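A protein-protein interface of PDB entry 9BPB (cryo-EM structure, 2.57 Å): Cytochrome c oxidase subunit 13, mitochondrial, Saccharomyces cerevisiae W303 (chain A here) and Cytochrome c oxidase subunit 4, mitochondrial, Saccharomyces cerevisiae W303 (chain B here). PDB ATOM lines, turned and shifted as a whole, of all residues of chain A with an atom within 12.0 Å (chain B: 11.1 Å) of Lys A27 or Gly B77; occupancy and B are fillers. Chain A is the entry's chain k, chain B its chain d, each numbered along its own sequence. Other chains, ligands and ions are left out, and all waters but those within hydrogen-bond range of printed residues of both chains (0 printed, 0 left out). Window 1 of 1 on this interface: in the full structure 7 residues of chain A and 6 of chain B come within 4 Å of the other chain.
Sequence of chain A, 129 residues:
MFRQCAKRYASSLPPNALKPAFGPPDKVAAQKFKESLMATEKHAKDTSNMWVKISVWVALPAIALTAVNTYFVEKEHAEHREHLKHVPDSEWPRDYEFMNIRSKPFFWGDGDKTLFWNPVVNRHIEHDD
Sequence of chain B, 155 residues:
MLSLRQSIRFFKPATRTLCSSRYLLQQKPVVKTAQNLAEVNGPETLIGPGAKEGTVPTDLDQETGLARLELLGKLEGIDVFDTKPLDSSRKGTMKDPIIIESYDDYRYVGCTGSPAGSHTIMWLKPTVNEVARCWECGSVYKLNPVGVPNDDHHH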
ATOM      1  N   PRO A  20      28.531  -9.990  14.661  1.00  0.00           N
ATOM      2  CA  PRO A  20      27.677 -10.668  13.673  1.00  0.00           C
ATOM      3  C   PRO A  20      26.283 -11.003  14.174  1.00  0.00           C
ATOM      4  O   PRO A  20      25.410 -11.295  13.347  1.00  0.00           O
ATOM      5  CB  PRO A  20      28.464 -11.942  13.346  1.00  0.00           C
ATOM      6  CG  PRO A  20      29.877 -11.597  13.646  1.00  0.00           C
ATOM      7  CD  PRO A  20      29.833 -10.662  14.821  1.00  0.00           C
ATOM      8  N   ALA A  21      26.051 -10.985  15.489  1.00  0.00           N
ATOM      9  CA  ALA A  21      24.760 -11.356  16.063  1.00  0.00           C
ATOM     10  C   ALA A  21      24.406 -12.789  15.695  1.00  0.00           C
ATOM     11  O   ALA A  21      24.829 -13.733  16.372  1.00  0.00           O
ATOM     12  CB  ALA A  21      23.656 -10.394  15.613  1.00  0.00           C
ATOM     13  N   PHE A  22      23.628 -12.963  14.630  1.00  0.00           N
ATOM     14  CA  PHE A  22      23.250 -14.299  14.195  1.00  0.00           C
ATOM     15  C   PHE A  22      24.460 -15.041  13.639  1.00  0.00           C
ATOM     16  O   PHE A  22      25.485 -14.446  13.303  1.00  0.00           O
ATOM     17  CB  PHE A  22      22.156 -14.224  13.132  1.00  0.00           C
ATOM     18  CG  PHE A  22      21.047 -13.279  13.477  1.00  0.00           C
ATOM     19  CD1 PHE A  22      20.141 -13.591  14.471  1.00  0.00           C
ATOM     20  CD2 PHE A  22      20.909 -12.079  12.804  1.00  0.00           C
ATOM     21  CE1 PHE A  22      19.123 -12.722  14.794  1.00  0.00           C
ATOM     22  CE2 PHE A  22      19.890 -11.208  13.121  1.00  0.00           C
ATOM     23  CZ  PHE A  22      18.995 -11.530  14.116  1.00  0.00           C
ATOM     24  N   GLY A  23      24.329 -16.360  13.539  1.00  0.00           N
ATOM     25  CA  GLY A  23      25.381 -17.187  12.999  1.00  0.00           C
ATOM     26  C   GLY A  23      25.386 -17.173  11.486  1.00  0.00           C
ATOM     27  O   GLY A  23      24.701 -16.367  10.849  1.00  0.00           O
ATOM     28  N   PRO A  24      26.167 -18.063  10.880  1.00  0.00           N
ATOM     29  CA  PRO A  24      26.208 -18.144   9.416  1.00  0.00           C
ATOM     30  C   PRO A  24      24.844 -18.493   8.853  1.00  0.00           C
ATOM     31  O   PRO A  24      24.104 -19.288   9.453  1.00  0.00           O
ATOM     32  CB  PRO A  24      27.227 -19.264   9.150  1.00  0.00           C
ATOM     33  CG  PRO A  24      27.240 -20.068  10.405  1.00  0.00           C
ATOM     34  CD  PRO A  24      27.013 -19.086  11.514  1.00  0.00           C
ATOM     35  N   PRO A  25      24.467 -17.911   7.715  1.00  0.00           N
ATOM     36  CA  PRO A  25      23.164 -18.232   7.120  1.00  0.00           C
ATOM     37  C   PRO A  25      23.050 -19.714   6.801  1.00  0.00           C
ATOM     38  O   PRO A  25      24.009 -20.349   6.357  1.00  0.00           O
ATOM     39  CB  PRO A  25      23.129 -17.375   5.847  1.00  0.00           C
ATOM     40  CG  PRO A  25      24.543 -16.944   5.614  1.00  0.00           C
ATOM     41  CD  PRO A  25      25.185 -16.875   6.958  1.00  0.00           C
ATOM     42  N   ASP A  26      21.858 -20.262   7.038  1.00  0.00           N
ATOM     43  CA  ASP A  26      21.642 -21.691   6.841  1.00  0.00           C
ATOM     44  C   ASP A  26      21.784 -22.076   5.372  1.00  0.00           C
ATOM     45  O   ASP A  26      22.442 -23.071   5.044  1.00  0.00           O
ATOM     46  CB  ASP A  26      20.266 -22.088   7.373  1.00  0.00           C
ATOM     47  CG  ASP A  26      20.189 -23.552   7.760  1.00  0.00           C
ATOM     48  OD1 ASP A  26      20.696 -24.400   6.997  1.00  0.00           O
ATOM     49  OD2 ASP A  26      19.621 -23.855   8.830  1.00  0.00           O
ATOM     50  N   LYS A  27      21.136 -21.321   4.481  1.00  0.00           N
ATOM     51  CA  LYS A  27      21.192 -21.525   3.034  1.00  0.00           C
ATOM     52  C   LYS A  27      20.496 -22.829   2.647  1.00  0.00           C
ATOM     53  O   LYS A  27      20.324 -23.126   1.460  1.00  0.00           O
ATOM     54  CB  LYS A  27      22.648 -21.486   2.543  1.00  0.00           C
ATOM     55  CG  LYS A  27      22.841 -21.571   1.036  1.00  0.00           C
ATOM     56  CD  LYS A  27      22.003 -20.533   0.307  1.00  0.00           C
ATOM     57  CE  LYS A  27      22.470 -19.121   0.612  1.00  0.00           C
ATOM     58  NZ  LYS A  27      21.676 -18.104  -0.133  1.00  0.00           N
ATOM     59  N   VAL A  28      20.056 -23.593   3.641  1.00  0.00           N
ATOM     60  CA  VAL A  28      19.283 -24.804   3.416  1.00  0.00           C
ATOM     61  C   VAL A  28      17.820 -24.605   3.792  1.00  0.00           C
ATOM     62  O   VAL A  28      16.928 -25.130   3.124  1.00  0.00           O
ATOM     63  CB  VAL A  28      19.906 -25.984   4.191  1.00  0.00           C
ATOM     64  CG1 VAL A  28      19.099 -27.255   3.975  1.00  0.00           C
ATOM     65  CG2 VAL A  28      21.350 -26.191   3.762  1.00  0.00           C
ATOM     66  N   ALA A  29      17.559 -23.843   4.857  1.00  0.00           N
ATOM     67  CA  ALA A  29      16.201 -23.372   5.103  1.00  0.00           C
ATOM     68  C   ALA A  29      15.725 -22.499   3.952  1.00  0.00           C
ATOM     69  O   ALA A  29      14.589 -22.636   3.485  1.00  0.00           O
ATOM     70  CB  ALA A  29      16.136 -22.611   6.427  1.00  0.00           C
ATOM     71  N   ALA A  30      16.581 -21.594   3.484  1.00  0.00           N
ATOM     72  CA  ALA A  30      16.378 -20.985   2.182  1.00  0.00           C
ATOM     73  C   ALA A  30      16.560 -22.038   1.094  1.00  0.00           C
ATOM     74  O   ALA A  30      17.334 -22.990   1.239  1.00  0.00           O
ATOM     75  CB  ALA A  30      17.348 -19.823   1.970  1.00  0.00           C
ATOM     76  N   GLN A  31      15.819 -21.865   0.001  1.00  0.00           N
ATOM     77  CA  GLN A  31      15.635 -22.797  -1.106  1.00  0.00           C
ATOM     78  C   GLN A  31      14.722 -23.951  -0.682  1.00  0.00           C
ATOM     79  O   GLN A  31      14.293 -24.726  -1.535  1.00  0.00           O
ATOM     80  CB  GLN A  31      16.962 -23.348  -1.669  1.00  0.00           C
ATOM     81  CG  GLN A  31      16.858 -24.184  -2.938  1.00  0.00           C
ATOM     82  CD  GLN A  31      16.884 -25.672  -2.657  1.00  0.00           C
ATOM     83  OE1 GLN A  31      17.540 -26.127  -1.719  1.00  0.00           O
ATOM     84  NE2 GLN A  31      16.167 -26.440  -3.467  1.00  0.00           N
ATOM     85  N   LYS A  32      14.377 -24.064   0.602  1.00  0.00           N
ATOM     86  CA  LYS A  32      13.256 -24.877   1.047  1.00  0.00           C
ATOM     87  C   LYS A  32      12.092 -24.040   1.543  1.00  0.00           C
ATOM     88  O   LYS A  32      10.968 -24.545   1.604  1.00  0.00           O
ATOM     89  CB  LYS A  32      13.693 -25.840   2.161  1.00  0.00           C
ATOM     90  CG  LYS A  32      14.586 -26.970   1.682  1.00  0.00           C
ATOM     91  CD  LYS A  32      14.895 -27.940   2.810  1.00  0.00           C
ATOM     92  CE  LYS A  32      15.675 -29.142   2.305  1.00  0.00           C
ATOM     93  NZ  LYS A  32      17.043 -28.770   1.860  1.00  0.00           N
ATOM     94  N   PHE A  33      12.340 -22.781   1.900  1.00  0.00           N
ATOM     95  CA  PHE A  33      11.288 -21.807   2.148  1.00  0.00           C
ATOM     96  C   PHE A  33      10.887 -21.070   0.879  1.00  0.00           C
ATOM     97  O   PHE A  33       9.707 -20.751   0.700  1.00  0.00           O
ATOM     98  CB  PHE A  33      11.750 -20.806   3.213  1.00  0.00           C
ATOM     99  CG  PHE A  33      10.919 -19.555   3.279  1.00  0.00           C
ATOM    100  CD1 PHE A  33       9.679 -19.560   3.891  1.00  0.00           C
ATOM    101  CD2 PHE A  33      11.388 -18.369   2.741  1.00  0.00           C
ATOM    102  CE1 PHE A  33       8.919 -18.408   3.956  1.00  0.00           C
ATOM    103  CE2 PHE A  33      10.631 -17.215   2.801  1.00  0.00           C
ATOM    104  CZ  PHE A  33       9.397 -17.235   3.409  1.00  0.00           C
ATOM    105  N   LYS A  34      11.846 -20.808  -0.012  1.00  0.00           N
ATOM    106  CA  LYS A  34      11.569 -20.075  -1.239  1.00  0.00           C
ATOM    107  C   LYS A  34      11.001 -20.955  -2.343  1.00  0.00           C
ATOM    108  O   LYS A  34      10.539 -20.424  -3.358  1.00  0.00           O
ATOM    109  CB  LYS A  34      12.839 -19.383  -1.736  1.00  0.00           C
ATOM    110  CG  LYS A  34      13.325 -18.258  -0.837  1.00  0.00           C
ATOM    111  CD  LYS A  34      14.719 -17.807  -1.232  1.00  0.00           C
ATOM    112  CE  LYS A  34      14.713 -17.138  -2.596  1.00  0.00           C
ATOM    113  NZ  LYS A  34      14.483 -15.670  -2.494  1.00  0.00           N
ATOM    114  N   GLU A  35      11.032 -22.276  -2.182  1.00  0.00           N
ATOM    115  CA  GLU A  35      10.392 -23.155  -3.152  1.00  0.00           C
ATOM    116  C   GLU A  35       8.996 -23.571  -2.717  1.00  0.00           C
ATOM    117  O   GLU A  35       8.146 -23.847  -3.572  1.00  0.00           O
ATOM    118  CB  GLU A  35      11.249 -24.402  -3.399  1.00  0.00           C
ATOM    119  CG  GLU A  35      11.331 -25.370  -2.228  1.00  0.00           C
ATOM    120  CD  GLU A  35      10.243 -26.426  -2.266  1.00  0.00           C
ATOM    121  OE1 GLU A  35       9.720 -26.701  -3.367  1.00  0.00           O
ATOM    122  OE2 GLU A  35       9.909 -26.979  -1.197  1.00  0.00           O
ATOM    123  N   SER A  36       8.742 -23.628  -1.406  1.00  0.00           N
ATOM    124  CA  SER A  36       7.395 -23.908  -0.925  1.00  0.00           C
ATOM    125  C   SER A  36       6.427 -22.805  -1.324  1.00  0.00           C
ATOM    126  O   SER A  36       5.252 -23.079  -1.594  1.00  0.00           O
ATOM    127  CB  SER A  36       7.404 -24.083   0.593  1.00  0.00           C
ATOM    128  OG  SER A  36       6.085 -24.077   1.113  1.00  0.00           O
ATOM    129  N   ASN B  36      17.914  -6.489   2.075  1.00  0.00           N
ATOM    130  CA  ASN B  36      18.740  -7.499   2.719  1.00  0.00           C
ATOM    131  C   ASN B  36      18.720  -7.253   4.220  1.00  0.00           C
ATOM    132  O   ASN B  36      18.398  -6.155   4.682  1.00  0.00           O
ATOM    133  CB  ASN B  36      20.176  -7.477   2.187  1.00  0.00           C
ATOM    134  CG  ASN B  36      20.894  -8.790   2.400  1.00  0.00           C
ATOM    135  OD1 ASN B  36      21.942  -8.844   3.041  1.00  0.00           O
ATOM    136  ND2 ASN B  36      20.330  -9.863   1.864  1.00  0.00           N
ATOM    137  N   LEU B  37      19.070  -8.294   4.978  1.00  0.00           N
ATOM    138  CA  LEU B  37      19.068  -8.170   6.432  1.00  0.00           C
ATOM    139  C   LEU B  37      20.240  -7.334   6.930  1.00  0.00           C
ATOM    140  O   LEU B  37      20.198  -6.816   8.050  1.00  0.00           O
ATOM    141  CB  LEU B  37      19.094  -9.556   7.072  1.00  0.00           C
ATOM    142  CG  LEU B  37      18.664  -9.642   8.536  1.00  0.00           C
ATOM    143  CD1 LEU B  37      17.199  -9.284   8.681  1.00  0.00           C
ATOM    144  CD2 LEU B  37      18.929 -11.030   9.076  1.00  0.00           C
ATOM    145  N   ALA B  38      21.289  -7.189   6.117  1.00  0.00           N
ATOM    146  CA  ALA B  38      22.457  -6.422   6.530  1.00  0.00           C
ATOM    147  C   ALA B  38      22.338  -4.944   6.188  1.00  0.00           C
ATOM    148  O   ALA B  38      23.239  -4.170   6.526  1.00  0.00           O
ATOM    149  CB  ALA B  38      23.717  -7.000   5.888  1.00  0.00           C
ATOM    150  N   LEU B  69      10.940  -7.266   8.937  1.00  0.00           N
ATOM    151  CA  LEU B  69      12.269  -7.693   9.360  1.00  0.00           C
ATOM    152  C   LEU B  69      12.321  -9.204   9.537  1.00  0.00           C
ATOM    153  O   LEU B  69      13.321  -9.844   9.188  1.00  0.00           O
ATOM    154  CB  LEU B  69      12.661  -6.980  10.652  1.00  0.00           C
ATOM    155  CG  LEU B  69      14.138  -6.988  11.045  1.00  0.00           C
ATOM    156  CD1 LEU B  69      14.506  -5.683  11.718  1.00  0.00           C
ATOM    157  CD2 LEU B  69      14.456  -8.154  11.961  1.00  0.00           C
ATOM    158  N   GLU B  70      11.252  -9.791  10.081  1.00  0.00           N
ATOM    159  CA  GLU B  70      11.159 -11.245  10.153  1.00  0.00           C
ATOM    160  C   GLU B  70      11.121 -11.864   8.762  1.00  0.00           C
ATOM    161  O   GLU B  70      11.739 -12.906   8.520  1.00  0.00           O
ATOM    162  CB  GLU B  70       9.923 -11.648  10.952  1.00  0.00           C
ATOM    163  CG  GLU B  70       9.719 -13.147  11.071  1.00  0.00           C
ATOM    164  CD  GLU B  70       8.461 -13.501  11.839  1.00  0.00           C
ATOM    165  OE1 GLU B  70       7.394 -12.939  11.521  1.00  0.00           O
ATOM    166  OE2 GLU B  70       8.540 -14.341  12.759  1.00  0.00           O
ATOM    167  N   LEU B  71      10.388 -11.240   7.836  1.00  0.00           N
ATOM    168  CA  LEU B  71      10.293 -11.768   6.479  1.00  0.00           C
ATOM    169  C   LEU B  71      11.642 -11.732   5.777  1.00  0.00           C
ATOM    170  O   LEU B  71      11.992 -12.663   5.042  1.00  0.00           O
ATOM    171  CB  LEU B  71       9.248 -10.983   5.686  1.00  0.00           C
ATOM    172  CG  LEU B  71       9.252 -11.155   4.167  1.00  0.00           C
ATOM    173  CD1 LEU B  71       8.673 -12.506   3.780  1.00  0.00           C
ATOM    174  CD2 LEU B  71       8.480 -10.032   3.502  1.00  0.00           C
ATOM    175  N   LEU B  72      12.415 -10.664   5.986  1.00  0.00           N
ATOM    176  CA  LEU B  72      13.743 -10.584   5.387  1.00  0.00           C
ATOM    177  C   LEU B  72      14.648 -11.694   5.903  1.00  0.00           C
ATOM    178  O   LEU B  72      15.453 -12.251   5.148  1.00  0.00           O
ATOM    179  CB  LEU B  72      14.364  -9.215   5.664  1.00  0.00           C
ATOM    180  CG  LEU B  72      13.862  -8.034   4.831  1.00  0.00           C
ATOM    181  CD1 LEU B  72      14.746  -6.815   5.040  1.00  0.00           C
ATOM    182  CD2 LEU B  72      13.801  -8.406   3.362  1.00  0.00           C
ATOM    183  N   GLY B  73      14.530 -12.028   7.190  1.00  0.00           N
ATOM    184  CA  GLY B  73      15.335 -13.101   7.746  1.00  0.00           C
ATOM    185  C   GLY B  73      15.016 -14.459   7.159  1.00  0.00           C
ATOM    186  O   GLY B  73      15.914 -15.288   6.986  1.00  0.00           O
ATOM    187  N   LYS B  74      13.743 -14.716   6.853  1.00  0.00           N
ATOM    188  CA  LYS B  74      13.360 -16.006   6.288  1.00  0.00           C
ATOM    189  C   LYS B  74      13.958 -16.227   4.905  1.00  0.00           C
ATOM    190  O   LYS B  74      14.280 -17.364   4.549  1.00  0.00           O
ATOM    191  CB  LYS B  74      11.837 -16.128   6.229  1.00  0.00           C
ATOM    192  CG  LYS B  74      11.171 -16.212   7.586  1.00  0.00           C
ATOM    193  CD  LYS B  74      11.478 -17.537   8.259  1.00  0.00           C
ATOM    194  CE  LYS B  74      10.794 -17.644   9.610  1.00  0.00           C
ATOM    195  NZ  LYS B  74      11.175 -18.891  10.325  1.00  0.00           N
ATOM    196  N   LEU B  75      14.104 -15.161   4.112  1.00  0.00           N
ATOM    197  CA  LEU B  75      14.656 -15.311   2.768  1.00  0.00           C
ATOM    198  C   LEU B  75      16.098 -15.797   2.819  1.00  0.00           C
ATOM    199  O   LEU B  75      16.564 -16.478   1.899  1.00  0.00           O
ATOM    200  CB  LEU B  75      14.551 -13.990   2.008  1.00  0.00           C
ATOM    201  CG  LEU B  75      13.138 -13.425   1.836  1.00  0.00           C
ATOM    202  CD1 LEU B  75      13.167 -12.103   1.088  1.00  0.00           C
ATOM    203  CD2 LEU B  75      12.241 -14.422   1.128  1.00  0.00           C
ATOM    204  N   GLU B  76      16.823 -15.446   3.877  1.00  0.00           N
ATOM    205  CA  GLU B  76      18.125 -16.030   4.147  1.00  0.00           C
ATOM    206  C   GLU B  76      17.967 -17.162   5.159  1.00  0.00           C
ATOM    207  O   GLU B  76      16.857 -17.523   5.561  1.00  0.00           O
ATOM    208  CB  GLU B  76      19.102 -14.967   4.651  1.00  0.00           C
ATOM    209  CG  GLU B  76      18.993 -13.620   3.952  1.00  0.00           C
ATOM    210  CD  GLU B  76      18.997 -13.740   2.441  1.00  0.00           C
ATOM    211  OE1 GLU B  76      19.924 -14.373   1.895  1.00  0.00           O
ATOM    212  OE2 GLU B  76      18.077 -13.195   1.796  1.00  0.00           O
ATOM    213  N   GLY B  77      19.085 -17.741   5.579  1.00  0.00           N
ATOM    214  CA  GLY B  77      19.031 -18.780   6.586  1.00  0.00           C
ATOM    215  C   GLY B  77      19.210 -18.240   7.989  1.00  0.00           C
ATOM    216  O   GLY B  77      20.156 -18.617   8.687  1.00  0.00           O
ATOM    217  N   ILE B  78      18.309 -17.361   8.415  1.00  0.00           N
ATOM    218  CA  ILE B  78      18.447 -16.659   9.685  1.00  0.00           C
ATOM    219  C   ILE B  78      17.101 -16.636  10.394  1.00  0.00           C
ATOM    220  O   ILE B  78      16.058 -16.420   9.768  1.00  0.00           O
ATOM    221  CB  ILE B  78      18.990 -15.230   9.471  1.00  0.00           C
ATOM    222  CG1 ILE B  78      20.514 -15.256   9.358  1.00  0.00           C
ATOM    223  CG2 ILE B  78      18.558 -14.307  10.596  1.00  0.00           C
ATOM    224  CD1 ILE B  78      21.102 -14.009   8.738  1.00  0.00           C
ATOM    225  N   ASP B  79      17.126 -16.874  11.703  1.00  0.00           N
ATOM    226  CA  ASP B  79      15.961 -16.725  12.569  1.00  0.00           C
ATOM    227  C   ASP B  79      16.229 -15.534  13.481  1.00  0.00           C
ATOM    228  O   ASP B  79      17.118 -15.590  14.336  1.00  0.00           O
ATOM    229  CB  ASP B  79      15.706 -18.000  13.369  1.00  0.00           C
ATOM    230  CG  ASP B  79      14.374 -17.981  14.093  1.00  0.00           C
ATOM    231  OD1 ASP B  79      13.653 -16.966  14.000  1.00  0.00           O
ATOM    232  OD2 ASP B  79      14.047 -18.986  14.759  1.00  0.00           O
ATOM    233  N   VAL B  80      15.465 -14.457  13.289  1.00  0.00           N
ATOM    234  CA  VAL B  80      15.741 -13.211  13.999  1.00  0.00           C
ATOM    235  C   VAL B  80      15.382 -13.336  15.475  1.00  0.00           C
ATOM    236  O   VAL B  80      15.903 -12.595  16.317  1.00  0.00           O
ATOM    237  CB  VAL B  80      15.000 -12.040  13.333  1.00  0.00           C
ATOM    238  CG1 VAL B  80      15.694 -11.642  12.044  1.00  0.00           C
ATOM    239  CG2 VAL B  80      13.554 -12.415  13.067  1.00  0.00           C
ATOM    240  N   PHE B  81      14.492 -14.261  15.814  1.00  0.00           N
ATOM    241  CA  PHE B  81      14.097 -14.494  17.195  1.00  0.00           C
ATOM    242  C   PHE B  81      14.651 -15.834  17.663  1.00  0.00           C
ATOM    243  O   PHE B  81      14.465 -16.855  16.997  1.00  0.00           O
ATOM    244  CB  PHE B  81      12.576 -14.454  17.338  1.00  0.00           C
ATOM    245  CG  PHE B  81      11.952 -13.217  16.763  1.00  0.00           C
ATOM    246  CD1 PHE B  81      12.476 -11.967  17.049  1.00  0.00           C
ATOM    247  CD2 PHE B  81      10.847 -13.297  15.936  1.00  0.00           C
ATOM    248  CE1 PHE B  81      11.911 -10.824  16.523  1.00  0.00           C
ATOM    249  CE2 PHE B  81      10.275 -12.155  15.403  1.00  0.00           C
ATOM    250  CZ  PHE B  81      10.809 -10.919  15.699  1.00  0.00           C
ATOM    251  N   LYS B  84      16.234 -21.221  21.117  1.00  0.00           N
ATOM    252  CA  LYS B  84      17.024 -22.392  21.482  1.00  0.00           C
ATOM    253  C   LYS B  84      17.205 -22.457  22.994  1.00  0.00           C
ATOM    254  O   LYS B  84      17.614 -21.466  23.607  1.00  0.00           O
ATOM    255  CB  LYS B  84      18.389 -22.355  20.806  1.00  0.00           C
ATOM    256  CG  LYS B  84      18.338 -22.364  19.293  1.00  0.00           C
ATOM    257  CD  LYS B  84      19.738 -22.285  18.708  1.00  0.00           C
ATOM    258  CE  LYS B  84      20.392 -20.950  19.029  1.00  0.00           C
ATOM    259  NZ  LYS B  84      19.649 -19.807  18.432  1.00  0.00           N
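The backbone carbonyl oxygen (O) of Gly B77 is in hydrogen-bond range of the backbone NH (N) of Asp A26.
The backbone carbonyl oxygen (O) of Gly B73 lies within hydrogen-bond range of the backbone NH (N) of Ile B78 (3.5 Å).
OD1 of Asp B79 sits close to N of Phe B81 (3.4 Å).
Among the printed residues, pairs that only touch across the chains: Pro A25 with Gly B77 (3.4 Å), Ala A30 with Leu B75 (3.4 Å), Phe A22 with Val B80 (3.5 Å), Phe A22 with Asp B79 (3.5 Å), Phe A33 with Lys B74 (3.6 Å), Phe A33 with Leu B75 (3.6 Å), Lys A34 with Leu B75 (3.9 Å), Lys A27 with Gly B77 (3.9 Å) and Phe A22 with Ile B78 (3.9 Å).
Of chain B, only Gly B77 comes within 4 Å of Lys A27.
Gly B77 touches three residues of chain A.
No residue of chain B comes within 4 Å of Gly A23.
Pro A25 touches one residue of chain B.
Of the printed residues of chain B, Asp A26 touches Gly B77 (2.9 Å).
No residue of chain B comes within 4 Å of Val A28.
No residue of chain B comes within 4 Å of Ala A29.
No residue of chain A comes within 4 Å of Glu B76.
Ile B78 touches just one residue of chain A: Phe A22 (3.9 Å).
Of the printed residues of chain A, Leu B75 touches Ala A30, Phe A33 and Lys A34.
Printed residues of chain B within 4 Å of Phe A22: Ile B78, Asp B79 and Val B80.
Ala B38 touches none of the printed residues of chain A.
Leu B69 touches none of the printed residues of chain A.
The nearest printed residue of chain B that does not touch Phe A33 is Leu B71 (4.8 Å).
Printed residues of chain A that touch a printed residue of chain B: Phe A22, Pro A25, Asp A26, Lys A27, Ala A30, Phe A33 and Lys A34.
Hydrophobic or aromatic side chains of chain A that line the printed part of chain B: Phe A22, Ala A30 and Phe A33.
Of the 17 printed residues of chain B, 6 touch a printed residue of chain A.
Hydrophobic or aromatic side chains of chain B that line the printed part of chain A: Leu B75, Ile B78 and Val B80.
Among the printed residues, 10 pairs touch across the chains.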
